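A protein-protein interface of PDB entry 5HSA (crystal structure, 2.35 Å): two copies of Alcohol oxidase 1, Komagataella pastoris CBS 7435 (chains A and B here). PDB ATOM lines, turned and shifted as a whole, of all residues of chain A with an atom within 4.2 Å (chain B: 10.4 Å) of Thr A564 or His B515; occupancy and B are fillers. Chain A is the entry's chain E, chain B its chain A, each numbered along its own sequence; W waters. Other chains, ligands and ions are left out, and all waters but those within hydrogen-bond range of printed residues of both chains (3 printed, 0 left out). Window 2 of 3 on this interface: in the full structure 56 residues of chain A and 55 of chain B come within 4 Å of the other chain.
Of the 14 printed residues of chain B, 4 touch a printed residue of chain A. Printed residues of chain B that touch a printed residue of chain A: His B515, Gly B516, Ser B517 and Trp B518. Hydrophobic or aromatic side chains of chain B within 4 Å of the printed part of chain A: His B515 and Trp B518. Printed residues of chain A that touch a printed residue of chain B: Phe A313, Glu A563, Thr A564 and Trp A566. Among the printed residues, 7 pairs touch across the chains.
Among the printed residues, pairs that only touch across the chains: Phe A313 with Trp B518, Trp A566 with His B515, Glu A563 with His B515 and Phe A313 with His B515.
No residue of chain B comes within 4 Å of Pro A85. Printed residues of chain B within 4 Å of Phe A313: His B515 and Trp B518. Glu A563 touches just these residues of chain B: His B515, Gly B516 and Ser B517. Thr A564 touches just one residue of chain B: His B515 (3.0 Å). Gly B512 touches none of the printed residues of chain A. His B515 touches just these residues of chain A: Phe A313, Glu A563, Thr A564 and Trp A566. Of the printed residues of chain A, Ser B517 touches Glu A563 (2.6 Å).
No position is printed for both chains. Of the 7 pairs that touch across the chains among the printed residues, none has its exchanged pair printed and touching as well.
NE2 of His B515 sits at hydrogen-bond distance from O of Thr A564 (3.0 Å). N of Gly B516 is in hydrogen-bond range of OE2 of Glu A563, 2.7 Å away. OG of Ser B517 is in hydrogen-bond range of OE2 of Glu A563, at 2.6 Å.
Water W1 lies within hydrogen-bond range of the side-chain carboxylate of Glu A563 (2.7 Å), the backbone NH of Ile A83 (2.9 Å) and the side-chain hydroxyl of Ser B517 (3.2 Å). Water W3 bridges a ring nitrogen (ND1) of His B515 (2.9 Å) and the backbone carbonyl oxygen (O) of Ile A83 (3.0 Å). Water W2 lies within hydrogen-bond range of the side-chain carboxylate of Glu A563 (3.0 Å) and the backbone carbonyl oxygen of Ala B514 (3.3 Å).
The side-chain hydroxyl of Tyr B486 lies within hydrogen-bond range of the backbone carbonyl oxygen of Ser B517 (2.6 Å). The side-chain hydroxyl (OG1) of Thr A564 lies within hydrogen-bond range of the side-chain carboxylate (OD2) of Asp A308. The backbone NH (N) of Glu A563 is in hydrogen-bond range of the backbone carbonyl oxygen (O) of Cys A311 (2.9 Å). O of Thr A564 sits at hydrogen-bond distance from SG of Cys A311 (3.4 Å). The backbone NH of Trp A566 sits at hydrogen-bond distance from the side-chain hydroxyl of Thr A564 (2.9 Å). The side-chain hydroxyl (OG1) of Thr A564 sits at hydrogen-bond distance from the side-chain sulfur (SG) of Cys A568 (3.8 Å).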
ATOM      1  N   ILE A  83     -21.244 -30.656  18.694  1.00  0.00           N
ATOM      2  CA  ILE A  83     -20.480 -29.605  18.041  1.00  0.00           C
ATOM      3  C   ILE A  83     -21.249 -28.297  18.134  1.00  0.00           C
ATOM      4  O   ILE A  83     -22.418 -28.225  17.753  1.00  0.00           O
ATOM      5  CB  ILE A  83     -20.196 -29.939  16.570  1.00  0.00           C
ATOM      6  CG1 ILE A  83     -19.397 -31.238  16.465  1.00  0.00           C
ATOM      7  CG2 ILE A  83     -19.444 -28.796  15.896  1.00  0.00           C
ATOM      8  CD1 ILE A  83     -19.154 -31.690  15.024  1.00  0.00           C
ATOM      9  N   VAL A  84     -20.594 -27.268  18.657  1.00  0.00           N
ATOM     10  CA  VAL A  84     -21.236 -25.971  18.828  1.00  0.00           C
ATOM     11  C   VAL A  84     -20.586 -24.938  17.925  1.00  0.00           C
ATOM     12  O   VAL A  84     -19.514 -24.417  18.234  1.00  0.00           O
ATOM     13  CB  VAL A  84     -21.169 -25.486  20.292  1.00  0.00           C
ATOM     14  CG1 VAL A  84     -21.894 -24.157  20.449  1.00  0.00           C
ATOM     15  CG2 VAL A  84     -21.767 -26.527  21.213  1.00  0.00           C
ATOM     16  N   PRO A  85     -21.228 -24.652  16.788  1.00  0.00           N
ATOM     17  CA  PRO A  85     -20.710 -23.647  15.861  1.00  0.00           C
ATOM     18  C   PRO A  85     -20.998 -22.232  16.345  1.00  0.00           C
ATOM     19  O   PRO A  85     -21.940 -22.018  17.119  1.00  0.00           O
ATOM     20  CB  PRO A  85     -21.472 -23.938  14.557  1.00  0.00           C
ATOM     21  CG  PRO A  85     -22.173 -25.264  14.773  1.00  0.00           C
ATOM     22  CD  PRO A  85     -22.417 -25.330  16.247  1.00  0.00           C
ATOM     23  N   ASP A 308     -28.492 -21.885  26.571  1.00  0.00           N
ATOM     24  CA  ASP A 308     -28.739 -21.936  25.136  1.00  0.00           C
ATOM     25  C   ASP A 308     -30.184 -22.332  24.913  1.00  0.00           C
ATOM     26  O   ASP A 308     -30.904 -22.638  25.860  1.00  0.00           O
ATOM     27  CB  ASP A 308     -27.797 -22.937  24.458  1.00  0.00           C
ATOM     28  CG  ASP A 308     -27.602 -22.661  22.972  1.00  0.00           C
ATOM     29  OD1 ASP A 308     -28.440 -21.966  22.349  1.00  0.00           O
ATOM     30  OD2 ASP A 308     -26.597 -23.156  22.424  1.00  0.00           O
ATOM     31  N   HIS A 309     -30.609 -22.314  23.661  1.00  0.00           N
ATOM     32  CA  HIS A 309     -31.847 -22.965  23.279  1.00  0.00           C
ATOM     33  C   HIS A 309     -31.492 -24.305  22.645  1.00  0.00           C
ATOM     34  O   HIS A 309     -30.527 -24.403  21.880  1.00  0.00           O
ATOM     35  CB  HIS A 309     -32.649 -22.096  22.318  1.00  0.00           C
ATOM     36  CG  HIS A 309     -33.205 -20.861  22.950  1.00  0.00           C
ATOM     37  ND1 HIS A 309     -33.313 -19.665  22.278  1.00  0.00           N
ATOM     38  CD2 HIS A 309     -33.688 -20.640  24.195  1.00  0.00           C
ATOM     39  CE1 HIS A 309     -33.841 -18.757  23.080  1.00  0.00           C
ATOM     40  NE2 HIS A 309     -34.077 -19.323  24.250  1.00  0.00           N
ATOM     41  N   CYS A 311     -32.352 -27.244  20.152  1.00  0.00           N
ATOM     42  CA  CYS A 311     -33.183 -27.424  18.966  1.00  0.00           C
ATOM     43  C   CYS A 311     -33.086 -28.821  18.354  1.00  0.00           C
ATOM     44  O   CYS A 311     -32.182 -29.587  18.669  1.00  0.00           O
ATOM     45  CB  CYS A 311     -32.818 -26.379  17.905  1.00  0.00           C
ATOM     46  SG  CYS A 311     -31.280 -26.671  16.991  1.00  0.00           S
ATOM     47  N   PHE A 313     -34.491 -30.896  14.357  1.00  0.00           N
ATOM     48  CA  PHE A 313     -35.141 -30.766  13.056  1.00  0.00           C
ATOM     49  C   PHE A 313     -35.861 -32.054  12.680  1.00  0.00           C
ATOM     50  O   PHE A 313     -35.321 -33.148  12.865  1.00  0.00           O
ATOM     51  CB  PHE A 313     -34.107 -30.409  11.983  1.00  0.00           C
ATOM     52  CG  PHE A 313     -33.397 -29.108  12.231  1.00  0.00           C
ATOM     53  CD1 PHE A 313     -32.337 -29.038  13.124  1.00  0.00           C
ATOM     54  CD2 PHE A 313     -33.797 -27.950  11.579  1.00  0.00           C
ATOM     55  CE1 PHE A 313     -31.692 -27.832  13.366  1.00  0.00           C
ATOM     56  CE2 PHE A 313     -33.153 -26.746  11.808  1.00  0.00           C
ATOM     57  CZ  PHE A 313     -32.099 -26.687  12.704  1.00  0.00           C
ATOM     58  N   PHE A 446     -26.236 -29.629  27.466  1.00  0.00           N
ATOM     59  CA  PHE A 446     -27.491 -29.922  26.770  1.00  0.00           C
ATOM     60  C   PHE A 446     -28.215 -31.111  27.397  1.00  0.00           C
ATOM     61  O   PHE A 446     -27.647 -32.195  27.516  1.00  0.00           O
ATOM     62  CB  PHE A 446     -27.236 -30.196  25.283  1.00  0.00           C
ATOM     63  CG  PHE A 446     -26.632 -29.034  24.538  1.00  0.00           C
ATOM     64  CD1 PHE A 446     -26.803 -27.732  24.986  1.00  0.00           C
ATOM     65  CD2 PHE A 446     -25.891 -29.247  23.384  1.00  0.00           C
ATOM     66  CE1 PHE A 446     -26.248 -26.665  24.301  1.00  0.00           C
ATOM     67  CE2 PHE A 446     -25.332 -28.181  22.691  1.00  0.00           C
ATOM     68  CZ  PHE A 446     -25.510 -26.891  23.149  1.00  0.00           C
ATOM     69  N   GLU A 563     -29.386 -30.146  19.150  1.00  0.00           N
ATOM     70  CA  GLU A 563     -28.195 -29.339  18.910  1.00  0.00           C
ATOM     71  C   GLU A 563     -28.337 -27.965  19.551  1.00  0.00           C
ATOM     72  O   GLU A 563     -29.420 -27.583  19.991  1.00  0.00           O
ATOM     73  CB  GLU A 563     -27.944 -29.162  17.405  1.00  0.00           C
ATOM     74  CG  GLU A 563     -27.942 -30.436  16.593  1.00  0.00           C
ATOM     75  CD  GLU A 563     -26.575 -31.089  16.544  1.00  0.00           C
ATOM     76  OE1 GLU A 563     -25.780 -30.878  17.491  1.00  0.00           O
ATOM     77  OE2 GLU A 563     -26.301 -31.805  15.553  1.00  0.00           O
ATOM     78  N   THR A 564     -27.236 -27.226  19.594  1.00  0.00           N
ATOM     79  CA  THR A 564     -27.293 -25.809  19.910  1.00  0.00           C
ATOM     80  C   THR A 564     -28.155 -25.102  18.866  1.00  0.00           C
ATOM     81  O   THR A 564     -28.182 -25.505  17.701  1.00  0.00           O
ATOM     82  CB  THR A 564     -25.894 -25.170  19.932  1.00  0.00           C
ATOM     83  OG1 THR A 564     -26.016 -23.763  20.175  1.00  0.00           O
ATOM     84  CG2 THR A 564     -25.187 -25.379  18.596  1.00  0.00           C
ATOM     85  N   THR A 565     -28.872 -24.064  19.282  1.00  0.00           N
ATOM     86  CA  THR A 565     -29.615 -23.236  18.338  1.00  0.00           C
ATOM     87  C   THR A 565     -28.818 -21.949  18.093  1.00  0.00           C
ATOM     88  O   THR A 565     -29.339 -20.961  17.557  1.00  0.00           O
ATOM     89  CB  THR A 565     -31.038 -22.909  18.853  1.00  0.00           C
ATOM     90  OG1 THR A 565     -31.571 -24.045  19.546  1.00  0.00           O
ATOM     91  CG2 THR A 565     -31.974 -22.562  17.702  1.00  0.00           C
ATOM     92  N   TRP A 566     -27.545 -21.984  18.492  1.00  0.00           N
ATOM     93  CA  TRP A 566     -26.628 -20.856  18.332  1.00  0.00           C
ATOM     94  C   TRP A 566     -27.045 -19.627  19.142  1.00  0.00           C
ATOM     95  O   TRP A 566     -26.602 -18.514  18.849  1.00  0.00           O
ATOM     96  CB  TRP A 566     -26.500 -20.455  16.854  1.00  0.00           C
ATOM     97  CG  TRP A 566     -26.213 -21.582  15.891  1.00  0.00           C
ATOM     98  CD1 TRP A 566     -25.018 -22.200  15.692  1.00  0.00           C
ATOM     99  CD2 TRP A 566     -27.139 -22.198  14.983  1.00  0.00           C
ATOM    100  NE1 TRP A 566     -25.141 -23.174  14.726  1.00  0.00           N
ATOM    101  CE2 TRP A 566     -26.432 -23.190  14.274  1.00  0.00           C
ATOM    102  CE3 TRP A 566     -28.496 -22.009  14.705  1.00  0.00           C
ATOM    103  CZ2 TRP A 566     -27.035 -23.992  13.301  1.00  0.00           C
ATOM    104  CZ3 TRP A 566     -29.099 -22.806  13.736  1.00  0.00           C
ATOM    105  CH2 TRP A 566     -28.366 -23.786  13.046  1.00  0.00           C
ATOM    106  N   CYS A 568     -26.451 -19.174  22.400  1.00  0.00           N
ATOM    107  CA  CYS A 568     -25.703 -19.300  23.651  1.00  0.00           C
ATOM    108  C   CYS A 568     -25.624 -17.985  24.436  1.00  0.00           C
ATOM    109  O   CYS A 568     -25.408 -16.922  23.856  1.00  0.00           O
ATOM    110  CB  CYS A 568     -24.292 -19.810  23.360  1.00  0.00           C
ATOM    111  SG  CYS A 568     -24.223 -21.063  22.079  1.00  0.00           S
ATOM    112  N   TYR B 486     -26.143 -44.993  19.447  1.00  0.00           N
ATOM    113  CA  TYR B 486     -25.577 -43.866  18.714  1.00  0.00           C
ATOM    114  C   TYR B 486     -24.061 -43.748  18.846  1.00  0.00           C
ATOM    115  O   TYR B 486     -23.377 -43.479  17.860  1.00  0.00           O
ATOM    116  CB  TYR B 486     -26.216 -42.545  19.159  1.00  0.00           C
ATOM    117  CG  TYR B 486     -25.917 -41.410  18.203  1.00  0.00           C
ATOM    118  CD1 TYR B 486     -24.709 -40.717  18.269  1.00  0.00           C
ATOM    119  CD2 TYR B 486     -26.827 -41.054  17.214  1.00  0.00           C
ATOM    120  CE1 TYR B 486     -24.418 -39.696  17.381  1.00  0.00           C
ATOM    121  CE2 TYR B 486     -26.547 -40.028  16.322  1.00  0.00           C
ATOM    122  CZ  TYR B 486     -25.341 -39.352  16.416  1.00  0.00           C
ATOM    123  OH  TYR B 486     -25.054 -38.332  15.543  1.00  0.00           O
ATOM    124  N   LEU B 497     -16.286 -35.867   4.665  1.00  0.00           N
ATOM    125  CA  LEU B 497     -16.594 -34.550   4.123  1.00  0.00           C
ATOM    126  C   LEU B 497     -16.205 -34.412   2.647  1.00  0.00           C
ATOM    127  O   LEU B 497     -17.007 -33.969   1.821  1.00  0.00           O
ATOM    128  CB  LEU B 497     -15.891 -33.464   4.943  1.00  0.00           C
ATOM    129  CG  LEU B 497     -16.155 -32.066   4.393  1.00  0.00           C
ATOM    130  CD1 LEU B 497     -17.419 -31.498   5.008  1.00  0.00           C
ATOM    131  CD2 LEU B 497     -14.972 -31.151   4.625  1.00  0.00           C
ATOM    132  N   SER B 510     -24.929 -27.551   1.006  1.00  0.00           N
ATOM    133  CA  SER B 510     -25.201 -28.230   2.275  1.00  0.00           C
ATOM    134  C   SER B 510     -24.417 -29.534   2.498  1.00  0.00           C
ATOM    135  O   SER B 510     -24.603 -30.194   3.526  1.00  0.00           O
ATOM    136  CB  SER B 510     -26.703 -28.523   2.405  1.00  0.00           C
ATOM    137  OG  SER B 510     -27.101 -29.647   1.618  1.00  0.00           O
ATOM    138  N   ALA B 511     -23.557 -29.919   1.559  1.00  0.00           N
ATOM    139  CA  ALA B 511     -22.722 -31.103   1.784  1.00  0.00           C
ATOM    140  C   ALA B 511     -21.795 -30.860   2.970  1.00  0.00           C
ATOM    141  O   ALA B 511     -21.084 -29.858   3.015  1.00  0.00           O
ATOM    142  CB  ALA B 511     -21.914 -31.457   0.537  1.00  0.00           C
ATOM    143  N   GLY B 512     -21.812 -31.768   3.937  1.00  0.00           N
ATOM    144  CA  GLY B 512     -20.986 -31.616   5.115  1.00  0.00           C
ATOM    145  C   GLY B 512     -21.598 -30.702   6.157  1.00  0.00           C
ATOM    146  O   GLY B 512     -20.927 -30.316   7.115  1.00  0.00           O
ATOM    147  N   LEU B 513     -22.866 -30.341   5.971  1.00  0.00           N
ATOM    148  CA  LEU B 513     -23.591 -29.588   6.992  1.00  0.00           C
ATOM    149  C   LEU B 513     -24.050 -30.568   8.058  1.00  0.00           C
ATOM    150  O   LEU B 513     -25.062 -31.242   7.886  1.00  0.00           O
ATOM    151  CB  LEU B 513     -24.780 -28.835   6.382  1.00  0.00           C
ATOM    152  CG  LEU B 513     -25.364 -27.600   7.089  1.00  0.00           C
ATOM    153  CD1 LEU B 513     -26.405 -26.928   6.199  1.00  0.00           C
ATOM    154  CD2 LEU B 513     -25.980 -27.937   8.440  1.00  0.00           C
ATOM    155  N   ALA B 514     -23.308 -30.644   9.160  1.00  0.00           N
ATOM    156  CA  ALA B 514     -23.492 -31.715  10.144  1.00  0.00           C
ATOM    157  C   ALA B 514     -24.654 -31.497  11.102  1.00  0.00           C
ATOM    158  O   ALA B 514     -25.137 -32.448  11.708  1.00  0.00           O
ATOM    159  CB  ALA B 514     -22.203 -31.913  10.949  1.00  0.00           C
ATOM    160  N   HIS B 515     -25.080 -30.247  11.257  1.00  0.00           N
ATOM    161  CA  HIS B 515     -26.124 -29.880  12.217  1.00  0.00           C
ATOM    162  C   HIS B 515     -27.374 -30.763  12.117  1.00  0.00           C
ATOM    163  O   HIS B 515     -28.020 -30.828  11.070  1.00  0.00           O
ATOM    164  CB  HIS B 515     -26.513 -28.417  12.019  1.00  0.00           C
ATOM    165  CG  HIS B 515     -26.841 -27.700  13.287  1.00  0.00           C
ATOM    166  ND1 HIS B 515     -25.889 -27.399  14.238  1.00  0.00           N
ATOM    167  CD2 HIS B 515     -28.014 -27.211  13.756  1.00  0.00           C
ATOM    168  CE1 HIS B 515     -26.463 -26.759  15.243  1.00  0.00           C
ATOM    169  NE2 HIS B 515     -27.751 -26.630  14.974  1.00  0.00           N
ATOM    170  N   GLY B 516     -27.706 -31.427  13.220  1.00  0.00           N
ATOM    171  CA  GLY B 516     -28.788 -32.397  13.255  1.00  0.00           C
ATOM    172  C   GLY B 516     -28.254 -33.751  13.701  1.00  0.00           C
ATOM    173  O   GLY B 516     -28.984 -34.559  14.283  1.00  0.00           O
ATOM    174  N   SER B 517     -26.970 -33.984  13.419  1.00  0.00           N
ATOM    175  CA  SER B 517     -26.256 -35.190  13.833  1.00  0.00           C
ATOM    176  C   SER B 517     -26.922 -36.461  13.304  1.00  0.00           C
ATOM    177  O   SER B 517     -27.017 -37.466  14.007  1.00  0.00           O
ATOM    178  CB  SER B 517     -26.137 -35.240  15.361  1.00  0.00           C
ATOM    179  OG  SER B 517     -25.291 -34.205  15.846  1.00  0.00           O
ATOM    180  N   TRP B 518     -27.371 -36.409  12.056  1.00  0.00           N
ATOM    181  CA  TRP B 518     -28.032 -37.547  11.437  1.00  0.00           C
ATOM    182  C   TRP B 518     -27.058 -38.681  11.131  1.00  0.00           C
ATOM    183  O   TRP B 518     -27.425 -39.856  11.178  1.00  0.00           O
ATOM    184  CB  TRP B 518     -28.763 -37.097  10.165  1.00  0.00           C
ATOM    185  CG  TRP B 518     -29.756 -36.012  10.465  1.00  0.00           C
ATOM    186  CD1 TRP B 518     -29.729 -34.722  10.010  1.00  0.00           C
ATOM    187  CD2 TRP B 518     -30.893 -36.110  11.329  1.00  0.00           C
ATOM    188  NE1 TRP B 518     -30.793 -34.020  10.521  1.00  0.00           N
ATOM    189  CE2 TRP B 518     -31.527 -34.853  11.336  1.00  0.00           C
ATOM    190  CE3 TRP B 518     -31.452 -37.146  12.087  1.00  0.00           C
ATOM    191  CZ2 TRP B 518     -32.682 -34.597  12.072  1.00  0.00           C
ATOM    192  CZ3 TRP B 518     -32.601 -36.893  12.820  1.00  0.00           C
ATOM    193  CH2 TRP B 518     -33.205 -35.627  12.802  1.00  0.00           C
ATOM    194  N   THR B 519     -25.814 -38.326  10.825  1.00  0.00           N
ATOM    195  CA  THR B 519     -24.791 -39.321  10.524  1.00  0.00           C
ATOM    196  C   THR B 519     -23.489 -38.985  11.237  1.00  0.00           C
ATOM    197  O   THR B 519     -23.320 -37.871  11.733  1.00  0.00           O
ATOM    198  CB  THR B 519     -24.503 -39.437   8.996  1.00  0.00           C
ATOM    199  OG1 THR B 519     -23.825 -38.259   8.544  1.00  0.00           O
ATOM    200  CG2 THR B 519     -25.794 -39.626   8.201  1.00  0.00           C
ATOM    201  N   GLN B 520     -22.584 -39.960  11.286  1.00  0.00           N
ATOM    202  CA  GLN B 520     -21.218 -39.750  11.746  1.00  0.00           C
ATOM    203  C   GLN B 520     -20.257 -40.187  10.636  1.00  0.00           C
ATOM    204  O   GLN B 520     -20.517 -41.167   9.939  1.00  0.00           O
ATOM    205  CB  GLN B 520     -20.951 -40.521  13.037  1.00  0.00           C
ATOM    206  CG  GLN B 520     -21.749 -40.021  14.233  1.00  0.00           C
ATOM    207  CD  GLN B 520     -21.331 -38.622  14.680  1.00  0.00           C
ATOM    208  OE1 GLN B 520     -20.145 -38.291  14.703  1.00  0.00           O
ATOM    209  NE2 GLN B 520     -22.310 -37.795  15.029  1.00  0.00           N
ATOM    210  N   PRO B 521     -19.151 -39.449  10.456  1.00  0.00           N
ATOM    211  CA  PRO B 521     -18.234 -39.665   9.336  1.00  0.00           C
ATOM    212  C   PRO B 521     -17.171 -40.733   9.570  1.00  0.00           C
ATOM    213  O   PRO B 521     -16.666 -40.910  10.676  1.00  0.00           O
ATOM    214  CB  PRO B 521     -17.569 -38.300   9.184  1.00  0.00           C
ATOM    215  CG  PRO B 521     -17.500 -37.791  10.582  1.00  0.00           C
ATOM    216  CD  PRO B 521     -18.765 -38.269  11.254  1.00  0.00           C
HETATM  217  O   HOH W   1     -23.334 -32.069  17.278  1.00  0.00           O
HETATM  218  O   HOH W   2     -23.492 -31.438  14.444  1.00  0.00           O
HETATM  219  O   HOH W   3     -23.406 -28.743  14.937  1.00  0.00           O
